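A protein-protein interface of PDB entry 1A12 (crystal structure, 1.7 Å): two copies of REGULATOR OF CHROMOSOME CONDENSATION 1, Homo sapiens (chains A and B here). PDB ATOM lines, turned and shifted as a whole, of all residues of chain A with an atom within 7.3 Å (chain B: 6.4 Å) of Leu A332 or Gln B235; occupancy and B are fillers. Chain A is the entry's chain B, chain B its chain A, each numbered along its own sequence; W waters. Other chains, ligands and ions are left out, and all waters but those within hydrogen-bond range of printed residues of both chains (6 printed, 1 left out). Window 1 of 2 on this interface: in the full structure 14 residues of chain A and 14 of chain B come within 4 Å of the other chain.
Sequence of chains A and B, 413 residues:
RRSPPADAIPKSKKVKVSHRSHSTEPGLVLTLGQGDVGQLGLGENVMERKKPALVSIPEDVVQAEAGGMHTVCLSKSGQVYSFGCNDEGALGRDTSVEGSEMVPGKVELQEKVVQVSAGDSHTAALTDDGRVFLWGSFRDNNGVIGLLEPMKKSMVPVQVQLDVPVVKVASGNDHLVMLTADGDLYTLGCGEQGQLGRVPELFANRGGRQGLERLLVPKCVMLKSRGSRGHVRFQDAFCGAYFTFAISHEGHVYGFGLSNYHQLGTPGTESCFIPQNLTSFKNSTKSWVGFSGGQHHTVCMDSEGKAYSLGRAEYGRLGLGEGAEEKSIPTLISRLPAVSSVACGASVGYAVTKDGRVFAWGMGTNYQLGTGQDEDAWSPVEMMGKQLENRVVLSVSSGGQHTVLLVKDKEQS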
ATOM      1  N   SER A 284      14.836  29.697   0.665  1.00  0.00           N
ATOM      2  CA  SER A 284      15.370  29.567  -0.700  1.00  0.00           C
ATOM      3  C   SER A 284      15.736  30.986  -1.182  1.00  0.00           C
ATOM      4  O   SER A 284      16.889  31.366  -1.288  1.00  0.00           O
ATOM      5  CB  SER A 284      14.291  28.975  -1.610  1.00  0.00           C
ATOM      6  OG  SER A 284      13.686  27.837  -1.021  1.00  0.00           O
ATOM      7  N   THR A 285      14.695  31.770  -1.364  1.00  0.00           N
ATOM      8  CA  THR A 285      14.742  33.131  -1.871  1.00  0.00           C
ATOM      9  C   THR A 285      13.303  33.701  -1.701  1.00  0.00           C
ATOM     10  O   THR A 285      13.007  34.831  -1.998  1.00  0.00           O
ATOM     11  CB  THR A 285      15.133  33.190  -3.368  1.00  0.00           C
ATOM     12  OG1 THR A 285      14.720  31.986  -4.029  1.00  0.00           O
ATOM     13  CG2 THR A 285      16.634  33.388  -3.532  1.00  0.00           C
ATOM     14  N   LYS A 286      12.447  32.798  -1.228  1.00  0.00           N
ATOM     15  CA  LYS A 286      11.060  33.107  -0.973  1.00  0.00           C
ATOM     16  C   LYS A 286      10.850  33.559   0.471  1.00  0.00           C
ATOM     17  O   LYS A 286      11.162  32.820   1.409  1.00  0.00           O
ATOM     18  CB  LYS A 286      10.207  31.861  -1.207  1.00  0.00           C
ATOM     19  CG  LYS A 286      10.713  30.948  -2.301  1.00  0.00           C
ATOM     20  CD  LYS A 286      10.027  29.603  -2.222  1.00  0.00           C
ATOM     21  CE  LYS A 286      10.589  28.641  -3.238  1.00  0.00           C
ATOM     22  NZ  LYS A 286      10.459  29.196  -4.612  1.00  0.00           N
ATOM     23  N   ASP A 302       4.727  33.840  -1.348  1.00  0.00           N
ATOM     24  CA  ASP A 302       6.012  34.442  -0.958  1.00  0.00           C
ATOM     25  C   ASP A 302       5.971  35.935  -1.249  1.00  0.00           C
ATOM     26  O   ASP A 302       4.968  36.443  -1.738  1.00  0.00           O
ATOM     27  CB  ASP A 302       7.208  33.759  -1.649  1.00  0.00           C
ATOM     28  CG  ASP A 302       7.194  33.883  -3.180  1.00  0.00           C
ATOM     29  OD1 ASP A 302       6.439  34.697  -3.746  1.00  0.00           O
ATOM     30  OD2 ASP A 302       7.975  33.150  -3.812  1.00  0.00           O
ATOM     31  N   GLU A 304       7.544  37.379  -3.641  1.00  0.00           N
ATOM     32  CA  GLU A 304       7.784  37.662  -5.065  1.00  0.00           C
ATOM     33  C   GLU A 304       6.583  37.375  -5.933  1.00  0.00           C
ATOM     34  O   GLU A 304       6.733  37.037  -7.128  1.00  0.00           O
ATOM     35  CB  GLU A 304       9.005  36.883  -5.547  1.00  0.00           C
ATOM     36  CG  GLU A 304      10.279  37.303  -4.837  1.00  0.00           C
ATOM     37  CD  GLU A 304      11.429  36.338  -5.024  1.00  0.00           C
ATOM     38  OE1 GLU A 304      11.232  35.237  -5.585  1.00  0.00           O
ATOM     39  OE2 GLU A 304      12.545  36.682  -4.588  1.00  0.00           O
ATOM     40  N   GLY A 305       5.366  37.508  -5.403  1.00  0.00           N
ATOM     41  CA  GLY A 305       4.155  37.381  -6.190  1.00  0.00           C
ATOM     42  C   GLY A 305       3.814  35.971  -6.619  1.00  0.00           C
ATOM     43  O   GLY A 305       3.066  35.765  -7.600  1.00  0.00           O
ATOM     44  N   LYS A 306       4.284  34.981  -5.874  1.00  0.00           N
ATOM     45  CA  LYS A 306       4.035  33.580  -6.211  1.00  0.00           C
ATOM     46  C   LYS A 306       3.239  32.886  -5.115  1.00  0.00           C
ATOM     47  O   LYS A 306       3.537  33.043  -3.925  1.00  0.00           O
ATOM     48  CB  LYS A 306       5.355  32.847  -6.441  1.00  0.00           C
ATOM     49  CG  LYS A 306       5.985  33.107  -7.800  1.00  0.00           C
ATOM     50  CD  LYS A 306       7.433  32.656  -7.810  1.00  0.00           C
ATOM     51  CE  LYS A 306       8.282  33.604  -6.986  1.00  0.00           C
ATOM     52  NZ  LYS A 306       9.529  32.972  -6.491  1.00  0.00           N
ATOM     53  N   ALA A 307       2.299  32.044  -5.529  1.00  0.00           N
ATOM     54  CA  ALA A 307       1.518  31.253  -4.585  1.00  0.00           C
ATOM     55  C   ALA A 307       1.856  29.763  -4.752  1.00  0.00           C
ATOM     56  O   ALA A 307       2.335  29.346  -5.789  1.00  0.00           O
ATOM     57  CB  ALA A 307       0.032  31.484  -4.818  1.00  0.00           C
ATOM     58  N   TYR A 308       1.827  29.057  -3.628  1.00  0.00           N
ATOM     59  CA  TYR A 308       2.186  27.639  -3.601  1.00  0.00           C
ATOM     60  C   TYR A 308       1.105  26.866  -2.833  1.00  0.00           C
ATOM     61  O   TYR A 308       0.470  27.433  -1.941  1.00  0.00           O
ATOM     62  CB  TYR A 308       3.531  27.450  -2.879  1.00  0.00           C
ATOM     63  CG  TYR A 308       4.693  28.274  -3.411  1.00  0.00           C
ATOM     64  CD1 TYR A 308       4.740  29.657  -3.231  1.00  0.00           C
ATOM     65  CD2 TYR A 308       5.760  27.662  -4.070  1.00  0.00           C
ATOM     66  CE1 TYR A 308       5.820  30.410  -3.695  1.00  0.00           C
ATOM     67  CE2 TYR A 308       6.842  28.406  -4.537  1.00  0.00           C
ATOM     68  CZ  TYR A 308       6.867  29.777  -4.346  1.00  0.00           C
ATOM     69  OH  TYR A 308       7.933  30.512  -4.806  1.00  0.00           O
ATOM     70  N   SER A 309       1.011  25.562  -3.108  1.00  0.00           N
ATOM     71  CA  SER A 309       0.085  24.728  -2.366  1.00  0.00           C
ATOM     72  C   SER A 309       0.757  23.455  -1.865  1.00  0.00           C
ATOM     73  O   SER A 309       1.791  23.014  -2.363  1.00  0.00           O
ATOM     74  CB  SER A 309      -1.115  24.372  -3.246  1.00  0.00           C
ATOM     75  OG  SER A 309      -0.699  23.719  -4.434  1.00  0.00           O
ATOM     76  N   LEU A 318      -5.340  21.713  -4.877  1.00  0.00           N
ATOM     77  CA  LEU A 318      -3.971  22.240  -4.924  1.00  0.00           C
ATOM     78  C   LEU A 318      -3.784  23.209  -6.082  1.00  0.00           C
ATOM     79  O   LEU A 318      -2.835  24.007  -6.122  1.00  0.00           O
ATOM     80  CB  LEU A 318      -2.959  21.097  -5.038  1.00  0.00           C
ATOM     81  CG  LEU A 318      -2.917  20.096  -3.879  1.00  0.00           C
ATOM     82  CD1 LEU A 318      -1.816  19.078  -4.122  1.00  0.00           C
ATOM     83  CD2 LEU A 318      -2.685  20.827  -2.567  1.00  0.00           C
ATOM     84  N   GLY A 319      -4.649  23.110  -7.090  1.00  0.00           N
ATOM     85  CA  GLY A 319      -4.576  24.067  -8.214  1.00  0.00           C
ATOM     86  C   GLY A 319      -3.353  23.833  -9.072  1.00  0.00           C
ATOM     87  O   GLY A 319      -2.930  24.736  -9.814  1.00  0.00           O
ATOM     88  N   LEU A 320      -2.853  22.607  -9.109  1.00  0.00           N
ATOM     89  CA  LEU A 320      -1.663  22.248  -9.841  1.00  0.00           C
ATOM     90  C   LEU A 320      -1.914  21.544 -11.158  1.00  0.00           C
ATOM     91  O   LEU A 320      -0.972  20.982 -11.749  1.00  0.00           O
ATOM     92  CB  LEU A 320      -0.746  21.388  -8.964  1.00  0.00           C
ATOM     93  CG  LEU A 320      -0.259  21.994  -7.645  1.00  0.00           C
ATOM     94  CD1 LEU A 320       0.511  20.951  -6.857  1.00  0.00           C
ATOM     95  CD2 LEU A 320       0.608  23.217  -7.910  1.00  0.00           C
ATOM     96  N   ILE A 329       5.638  19.487   0.248  1.00  0.00           N
ATOM     97  CA  ILE A 329       6.448  20.702   0.246  1.00  0.00           C
ATOM     98  C   ILE A 329       5.670  21.764  -0.578  1.00  0.00           C
ATOM     99  O   ILE A 329       4.845  21.376  -1.401  1.00  0.00           O
ATOM    100  CB  ILE A 329       7.833  20.471  -0.418  1.00  0.00           C
ATOM    101  CG1 ILE A 329       7.673  20.035  -1.879  1.00  0.00           C
ATOM    102  CG2 ILE A 329       8.632  19.434   0.364  1.00  0.00           C
ATOM    103  CD1 ILE A 329       8.975  19.983  -2.653  1.00  0.00           C
ATOM    104  N   PRO A 330       5.863  23.021  -0.262  1.00  0.00           N
ATOM    105  CA  PRO A 330       5.163  24.095  -0.978  1.00  0.00           C
ATOM    106  C   PRO A 330       5.474  24.008  -2.466  1.00  0.00           C
ATOM    107  O   PRO A 330       6.640  23.970  -2.857  1.00  0.00           O
ATOM    108  CB  PRO A 330       5.734  25.365  -0.340  1.00  0.00           C
ATOM    109  CG  PRO A 330       7.076  24.929   0.182  1.00  0.00           C
ATOM    110  CD  PRO A 330       6.763  23.580   0.759  1.00  0.00           C
ATOM    111  N   THR A 331       4.420  23.837  -3.261  1.00  0.00           N
ATOM    112  CA  THR A 331       4.582  23.576  -4.698  1.00  0.00           C
ATOM    113  C   THR A 331       3.998  24.702  -5.523  1.00  0.00           C
ATOM    114  O   THR A 331       2.830  25.069  -5.358  1.00  0.00           O
ATOM    115  CB  THR A 331       3.909  22.251  -5.111  1.00  0.00           C
ATOM    116  OG1 THR A 331       4.421  21.185  -4.303  1.00  0.00           O
ATOM    117  CG2 THR A 331       4.192  21.936  -6.575  1.00  0.00           C
ATOM    118  N   LEU A 332       4.830  25.303  -6.365  1.00  0.00           N
ATOM    119  CA  LEU A 332       4.429  26.522  -7.077  1.00  0.00           C
ATOM    120  C   LEU A 332       3.201  26.319  -7.934  1.00  0.00           C
ATOM    121  O   LEU A 332       3.096  25.345  -8.696  1.00  0.00           O
ATOM    122  CB  LEU A 332       5.591  27.016  -7.947  1.00  0.00           C
ATOM    123  CG  LEU A 332       5.390  28.283  -8.783  1.00  0.00           C
ATOM    124  CD1 LEU A 332       5.117  29.470  -7.877  1.00  0.00           C
ATOM    125  CD2 LEU A 332       6.621  28.538  -9.636  1.00  0.00           C
ATOM    126  N   ILE A 333       2.244  27.244  -7.809  1.00  0.00           N
ATOM    127  CA  ILE A 333       1.057  27.252  -8.666  1.00  0.00           C
ATOM    128  C   ILE A 333       1.351  28.219  -9.834  1.00  0.00           C
ATOM    129  O   ILE A 333       1.245  29.432  -9.658  1.00  0.00           O
ATOM    130  CB  ILE A 333      -0.185  27.760  -7.913  1.00  0.00           C
ATOM    131  CG1 ILE A 333      -0.429  26.912  -6.665  1.00  0.00           C
ATOM    132  CG2 ILE A 333      -1.410  27.716  -8.823  1.00  0.00           C
ATOM    133  CD1 ILE A 333      -1.516  27.456  -5.766  1.00  0.00           C
ATOM    134  N   SER A 334       1.968  27.691 -10.883  1.00  0.00           N
ATOM    135  CA  SER A 334       2.583  28.522 -11.905  1.00  0.00           C
ATOM    136  C   SER A 334       1.572  29.264 -12.756  1.00  0.00           C
ATOM    137  O   SER A 334       1.907  30.283 -13.391  1.00  0.00           O
ATOM    138  CB  SER A 334       3.479  27.670 -12.805  1.00  0.00           C
ATOM    139  OG  SER A 334       2.724  26.686 -13.487  1.00  0.00           O
ATOM    140  N   ARG A 335       0.358  28.743 -12.860  1.00  0.00           N
ATOM    141  CA  ARG A 335      -0.651  29.256 -13.772  1.00  0.00           C
ATOM    142  C   ARG A 335      -1.263  30.575 -13.376  1.00  0.00           C
ATOM    143  O   ARG A 335      -2.121  31.087 -14.150  1.00  0.00           O
ATOM    144  CB  ARG A 335      -1.774  28.226 -13.935  1.00  0.00           C
ATOM    145  CG  ARG A 335      -1.365  26.902 -14.565  1.00  0.00           C
ATOM    146  CD  ARG A 335      -2.533  25.924 -14.527  1.00  0.00           C
ATOM    147  NE  ARG A 335      -2.305  24.721 -15.323  1.00  0.00           N
ATOM    148  CZ  ARG A 335      -1.629  23.653 -14.910  1.00  0.00           C
ATOM    149  NH1 ARG A 335      -1.095  23.621 -13.696  1.00  0.00           N
ATOM    150  NH2 ARG A 335      -1.494  22.605 -15.712  1.00  0.00           N
ATOM    151  N   HIS B  19       0.418  33.368 -16.308  1.00  0.00           N
ATOM    152  CA  HIS B  19       1.747  33.340 -15.713  1.00  0.00           C
ATOM    153  C   HIS B  19       2.058  34.772 -15.256  1.00  0.00           C
ATOM    154  O   HIS B  19       1.539  35.710 -15.860  1.00  0.00           O
ATOM    155  CB  HIS B  19       2.802  32.863 -16.714  1.00  0.00           C
ATOM    156  CG  HIS B  19       4.103  32.491 -16.080  1.00  0.00           C
ATOM    157  ND1 HIS B  19       5.240  33.265 -16.200  1.00  0.00           N
ATOM    158  CD2 HIS B  19       4.451  31.436 -15.305  1.00  0.00           C
ATOM    159  CE1 HIS B  19       6.230  32.699 -15.525  1.00  0.00           C
ATOM    160  NE2 HIS B  19       5.774  31.588 -14.974  1.00  0.00           N
ATOM    161  N   ARG B  20       2.948  34.895 -14.284  1.00  0.00           N
ATOM    162  CA  ARG B  20       3.257  36.234 -13.779  1.00  0.00           C
ATOM    163  C   ARG B  20       4.014  37.041 -14.825  1.00  0.00           C
ATOM    164  O   ARG B  20       4.061  38.264 -14.696  1.00  0.00           O
ATOM    165  CB  ARG B  20       4.032  36.153 -12.461  1.00  0.00           C
ATOM    166  CG  ARG B  20       5.283  35.300 -12.499  1.00  0.00           C
ATOM    167  CD  ARG B  20       5.790  35.053 -11.087  1.00  0.00           C
ATOM    168  NE  ARG B  20       7.067  34.340 -11.068  1.00  0.00           N
ATOM    169  CZ  ARG B  20       7.229  33.065 -11.408  1.00  0.00           C
ATOM    170  NH1 ARG B  20       6.194  32.333 -11.803  1.00  0.00           N
ATOM    171  NH2 ARG B  20       8.434  32.521 -11.345  1.00  0.00           N
ATOM    172  N   LEU B 179       8.675  26.952 -20.760  1.00  0.00           N
ATOM    173  CA  LEU B 179       8.567  26.511 -19.351  1.00  0.00           C
ATOM    174  C   LEU B 179       7.159  25.958 -19.135  1.00  0.00           C
ATOM    175  O   LEU B 179       6.193  26.651 -19.413  1.00  0.00           O
ATOM    176  CB  LEU B 179       8.801  27.690 -18.406  1.00  0.00           C
ATOM    177  CG  LEU B 179       8.657  27.410 -16.906  1.00  0.00           C
ATOM    178  CD1 LEU B 179       9.762  26.472 -16.440  1.00  0.00           C
ATOM    179  CD2 LEU B 179       8.707  28.717 -16.138  1.00  0.00           C
ATOM    180  N   ALA B 181       3.814  24.302 -17.149  1.00  0.00           N
ATOM    181  CA  ALA B 181       3.126  24.521 -15.895  1.00  0.00           C
ATOM    182  C   ALA B 181       3.761  23.728 -14.751  1.00  0.00           C
ATOM    183  O   ALA B 181       3.624  24.141 -13.593  1.00  0.00           O
ATOM    184  CB  ALA B 181       1.658  24.155 -16.036  1.00  0.00           C
ATOM    185  N   GLY B 183       6.984  23.138 -14.362  1.00  0.00           N
ATOM    186  CA  GLY B 183       8.337  23.587 -13.994  1.00  0.00           C
ATOM    187  C   GLY B 183       9.396  22.928 -14.855  1.00  0.00           C
ATOM    188  O   GLY B 183      10.593  23.032 -14.575  1.00  0.00           O
ATOM    189  N   ARG B 233      13.388  21.249 -11.056  1.00  0.00           N
ATOM    190  CA  ARG B 233      12.346  21.972 -11.802  1.00  0.00           C
ATOM    191  C   ARG B 233      12.500  23.466 -11.575  1.00  0.00           C
ATOM    192  O   ARG B 233      13.207  23.886 -10.656  1.00  0.00           O
ATOM    193  CB  ARG B 233      10.957  21.495 -11.374  1.00  0.00           C
ATOM    194  CG  ARG B 233      10.566  20.154 -11.973  1.00  0.00           C
ATOM    195  CD  ARG B 233       9.212  19.689 -11.469  1.00  0.00           C
ATOM    196  NE  ARG B 233       8.556  18.794 -12.424  1.00  0.00           N
ATOM    197  CZ  ARG B 233       8.954  17.556 -12.706  1.00  0.00           C
ATOM    198  NH1 ARG B 233      10.018  17.038 -12.105  1.00  0.00           N
ATOM    199  NH2 ARG B 233       8.293  16.840 -13.604  1.00  0.00           N
ATOM    200  N   PHE B 234      11.940  24.270 -12.473  1.00  0.00           N
ATOM    201  CA  PHE B 234      12.213  25.690 -12.543  1.00  0.00           C
ATOM    202  C   PHE B 234      11.005  26.577 -12.355  1.00  0.00           C
ATOM    203  O   PHE B 234       9.909  26.260 -12.810  1.00  0.00           O
ATOM    204  CB  PHE B 234      12.886  25.973 -13.887  1.00  0.00           C
ATOM    205  CG  PHE B 234      14.078  25.092 -14.164  1.00  0.00           C
ATOM    206  CD1 PHE B 234      15.329  25.422 -13.654  1.00  0.00           C
ATOM    207  CD2 PHE B 234      13.944  23.914 -14.898  1.00  0.00           C
ATOM    208  CE1 PHE B 234      16.434  24.598 -13.875  1.00  0.00           C
ATOM    209  CE2 PHE B 234      15.042  23.082 -15.127  1.00  0.00           C
ATOM    210  CZ  PHE B 234      16.291  23.428 -14.617  1.00  0.00           C
ATOM    211  N   GLN B 235      11.199  27.754 -11.751  1.00  0.00           N
ATOM    212  CA  GLN B 235      10.153  28.740 -11.579  1.00  0.00           C
ATOM    213  C   GLN B 235      10.182  29.822 -12.656  1.00  0.00           C
ATOM    214  O   GLN B 235       9.190  30.525 -12.867  1.00  0.00           O
ATOM    215  CB  GLN B 235      10.239  29.374 -10.189  1.00  0.00           C
ATOM    216  CG  GLN B 235      11.576  30.023  -9.872  1.00  0.00           C
ATOM    217  CD  GLN B 235      11.600  30.676  -8.505  1.00  0.00           C
ATOM    218  OE1 GLN B 235      10.951  31.692  -8.282  1.00  0.00           O
ATOM    219  NE2 GLN B 235      12.356  30.092  -7.582  1.00  0.00           N
ATOM    220  N   ASP B 236      11.307  29.953 -13.364  1.00  0.00           N
ATOM    221  CA  ASP B 236      11.403  30.923 -14.455  1.00  0.00           C
ATOM    222  C   ASP B 236      12.586  30.604 -15.372  1.00  0.00           C
ATOM    223  O   ASP B 236      13.423  29.756 -15.056  1.00  0.00           O
ATOM    224  CB  ASP B 236      11.537  32.336 -13.894  1.00  0.00           C
ATOM    225  CG  ASP B 236      10.778  33.359 -14.710  1.00  0.00           C
ATOM    226  OD1 ASP B 236      10.498  33.099 -15.900  1.00  0.00           O
ATOM    227  OD2 ASP B 236      10.452  34.430 -14.157  1.00  0.00           O
ATOM    228  N   ALA B 237      12.532  31.144 -16.588  1.00  0.00           N
ATOM    229  CA  ALA B 237      13.584  30.898 -17.578  1.00  0.00           C
ATOM    230  C   ALA B 237      13.647  32.073 -18.567  1.00  0.00           C
ATOM    231  O   ALA B 237      12.676  32.807 -18.686  1.00  0.00           O
ATOM    232  CB  ALA B 237      13.316  29.596 -18.322  1.00  0.00           C
ATOM    233  N   ALA B 246      18.037  29.740 -16.146  1.00  0.00           N
ATOM    234  CA  ALA B 246      16.830  29.143 -15.561  1.00  0.00           C
ATOM    235  C   ALA B 246      16.942  29.208 -14.030  1.00  0.00           C
ATOM    236  O   ALA B 246      17.996  28.921 -13.493  1.00  0.00           O
ATOM    237  CB  ALA B 246      16.684  27.692 -16.026  1.00  0.00           C
ATOM    238  N   ILE B 247      15.855  29.639 -13.401  1.00  0.00           N
ATOM    239  CA  ILE B 247      15.879  29.757 -11.934  1.00  0.00           C
ATOM    240  C   ILE B 247      15.065  28.608 -11.330  1.00  0.00           C
ATOM    241  O   ILE B 247      13.916  28.411 -11.717  1.00  0.00           O
ATOM    242  CB  ILE B 247      15.227  31.056 -11.480  1.00  0.00           C
ATOM    243  CG1 ILE B 247      15.884  32.237 -12.190  1.00  0.00           C
ATOM    244  CG2 ILE B 247      15.336  31.195  -9.968  1.00  0.00           C
ATOM    245  CD1 ILE B 247      15.170  33.541 -11.975  1.00  0.00           C
ATOM    246  N   SER B 248      15.725  27.786 -10.532  1.00  0.00           N
ATOM    247  CA  SER B 248      15.072  26.614  -9.945  1.00  0.00           C
ATOM    248  C   SER B 248      14.032  27.040  -8.919  1.00  0.00           C
ATOM    249  O   SER B 248      14.007  28.182  -8.481  1.00  0.00           O
ATOM    250  CB  SER B 248      16.085  25.645  -9.325  1.00  0.00           C
ATOM    251  OG  SER B 248      16.664  26.177  -8.149  1.00  0.00           O
ATOM    252  N   HIS B 249      13.244  26.059  -8.458  1.00  0.00           N
ATOM    253  CA  HIS B 249      12.247  26.337  -7.414  1.00  0.00           C
ATOM    254  C   HIS B 249      12.903  26.851  -6.127  1.00  0.00           C
ATOM    255  O   HIS B 249      12.303  27.644  -5.384  1.00  0.00           O
ATOM    256  CB  HIS B 249      11.359  25.119  -7.166  1.00  0.00           C
ATOM    257  CG  HIS B 249      10.324  24.914  -8.229  1.00  0.00           C
ATOM    258  ND1 HIS B 249       9.505  25.931  -8.671  1.00  0.00           N
ATOM    259  CD2 HIS B 249       9.992  23.821  -8.954  1.00  0.00           C
ATOM    260  CE1 HIS B 249       8.713  25.473  -9.625  1.00  0.00           C
ATOM    261  NE2 HIS B 249       8.989  24.195  -9.816  1.00  0.00           N
ATOM    262  N   GLU B 250      14.124  26.415  -5.903  1.00  0.00           N
ATOM    263  CA  GLU B 250      14.894  26.798  -4.706  1.00  0.00           C
ATOM    264  C   GLU B 250      15.530  28.187  -4.861  1.00  0.00           C
ATOM    265  O   GLU B 250      16.050  28.763  -3.897  1.00  0.00           O
ATOM    266  CB  GLU B 250      16.005  25.774  -4.458  1.00  0.00           C
ATOM    267  CG  GLU B 250      15.616  24.580  -3.597  1.00  0.00           C
ATOM    268  CD  GLU B 250      15.998  24.755  -2.132  1.00  0.00           C
ATOM    269  OE1 GLU B 250      16.818  25.650  -1.817  1.00  0.00           O
ATOM    270  OE2 GLU B 250      15.489  23.983  -1.288  1.00  0.00           O
ATOM    271  N   GLY B 251      15.509  28.701  -6.075  1.00  0.00           N
ATOM    272  CA  GLY B 251      16.023  30.053  -6.355  1.00  0.00           C
ATOM    273  C   GLY B 251      17.477  30.054  -6.855  1.00  0.00           C
ATOM    274  O   GLY B 251      18.123  31.110  -6.934  1.00  0.00           O
ATOM    275  N   HIS B 252      17.995  28.885  -7.187  1.00  0.00           N
ATOM    276  CA  HIS B 252      19.363  28.786  -7.736  1.00  0.00           C
ATOM    277  C   HIS B 252      19.333  29.124  -9.219  1.00  0.00           C
ATOM    278  O   HIS B 252      18.408  28.732  -9.942  1.00  0.00           O
ATOM    279  CB  HIS B 252      19.881  27.335  -7.617  1.00  0.00           C
ATOM    280  CG  HIS B 252      19.989  26.819  -6.213  1.00  0.00           C
ATOM    281  ND1 HIS B 252      19.664  25.522  -5.872  1.00  0.00           N
ATOM    282  CD2 HIS B 252      20.431  27.404  -5.075  1.00  0.00           C
ATOM    283  CE1 HIS B 252      19.902  25.332  -4.588  1.00  0.00           C
ATOM    284  NE2 HIS B 252      20.367  26.460  -4.081  1.00  0.00           N
ATOM    285  N   TRP B 288      17.338  36.699  -7.624  1.00  0.00           N
ATOM    286  CA  TRP B 288      17.348  37.023  -9.054  1.00  0.00           C
ATOM    287  C   TRP B 288      16.007  36.801  -9.711  1.00  0.00           C
ATOM    288  O   TRP B 288      15.388  35.737  -9.525  1.00  0.00           O
ATOM    289  CB  TRP B 288      18.389  36.177  -9.760  1.00  0.00           C
ATOM    290  CG  TRP B 288      19.699  36.421  -9.180  1.00  0.00           C
ATOM    291  CD1 TRP B 288      20.382  35.613  -8.325  1.00  0.00           C
ATOM    292  CD2 TRP B 288      20.470  37.612  -9.321  1.00  0.00           C
ATOM    293  NE1 TRP B 288      21.535  36.232  -7.912  1.00  0.00           N
ATOM    294  CE2 TRP B 288      21.614  37.462  -8.514  1.00  0.00           C
ATOM    295  CE3 TRP B 288      20.304  38.795 -10.055  1.00  0.00           C
ATOM    296  CZ2 TRP B 288      22.593  38.455  -8.411  1.00  0.00           C
ATOM    297  CZ3 TRP B 288      21.272  39.780  -9.955  1.00  0.00           C
ATOM    298  CH2 TRP B 288      22.406  39.602  -9.140  1.00  0.00           C
HETATM  299  O   HOH W   1       7.661  24.308  -6.655  1.00  0.00           O
HETATM  300  O   HOH W   2       1.573  24.694 -11.037  1.00  0.00           O
HETATM  301  O   HOH W   3      12.274  31.121  -4.814  1.00  0.00           O
HETATM  302  O   HOH W   4       1.593  22.177 -12.043  1.00  0.00           O
HETATM  303  O   HOH W   5       9.221  28.048  -6.956  1.00  0.00           O
HETATM  304  O   HOH W   6       3.168  32.527 -12.251  1.00  0.00           O
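OG of Ser A334 lies within hydrogen-bond range of O of Ala B181, 2.7 Å away. The side-chain amino group (NZ) of Lys A306 lies within hydrogen-bond range of the side-chain amide oxygen (OE1) of Gln B235 (2.6 Å). O of His B249 lies within hydrogen-bond range of NZ of Lys A286 (2.5 Å). The side-chain hydroxyl of Thr A285 lies within hydrogen-bond range of the backbone carbonyl oxygen of Glu B250, 3.5 Å away.
Among the printed residues, merely in contact across the chains: Ser A284 with Glu B250 (2.9 Å), Thr A285 with Gly B251 (3.3 Å), Ser A334 with His B19 (3.4 Å), Arg A335 with Ala B181 (3.5 Å), Lys A306 with Arg B20 (3.6 Å), Lys A286 with Gln B235 (3.6 Å), Leu A332 with His B249 (3.7 Å) and Leu A332 with Gln B235 (3.8 Å).
Hydrophobic or aromatic side chains of chain B that line the printed part of chain A: His B19, Ala B181 and His B249. Hydrophobic or aromatic side chains of chain A that line the printed part of chain B: Leu A332. Among the printed residues, 12 pairs touch across the chains.
The backbone carbonyl oxygen (O) of His B249 sits at hydrogen-bond distance from the side-chain amide nitrogen (NE2) of Gln B235. The side-chain carboxylate (OE1) of Glu A304 is in salt-bridge range of the side-chain amino group (NZ) of Lys A306. The side-chain hydroxyl (OH) of Tyr A308 is in hydrogen-bond range of the side-chain amino group (NZ) of Lys A306, 3.4 Å away.
No position is printed for both chains. Of the 12 pairs that touch across the chains among the printed residues, none has its exchanged pair printed and touching as well.
Of the printed residues of chain B, Thr A285 touches Glu B250 and Gly B251. Printed residues of chain B within 4 Å of Lys A306: Arg B20 (3.6 Å) and Gln B235 (2.6 Å). Leu A318 touches none of the printed residues of chain B. Leu A332 touches just these residues of chain B: Gln B235 (3.8 Å) and His B249 (3.7 Å). Printed residues of chain B within 4 Å of Ser A334: His B19 and Ala B181. Gln B235 touches just these residues of chain A: Lys A286 (3.6 Å), Lys A306 (2.6 Å) and Leu A332 (3.8 Å). The nearest residue of chain A that does not touch Gln B235 is Glu A304 (4.5 Å).
Water W5 bridges ND1 of His B249 (2.7 Å) and NZ of Lys A286 (2.9 Å). Water W6 lies within hydrogen-bond range of the backbone carbonyl oxygen (O) of Ser A334 and the guanidinium group (NH1) of Arg B20. Water W2 lies within hydrogen-bond range of O of Leu A332, N of Ser A334 and O of Ala B181. Water W1 lies within hydrogen-bond range of the backbone NH (N) of Leu A332 (3.0 Å) and a ring nitrogen (ND1) of His B249 (3.2 Å).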
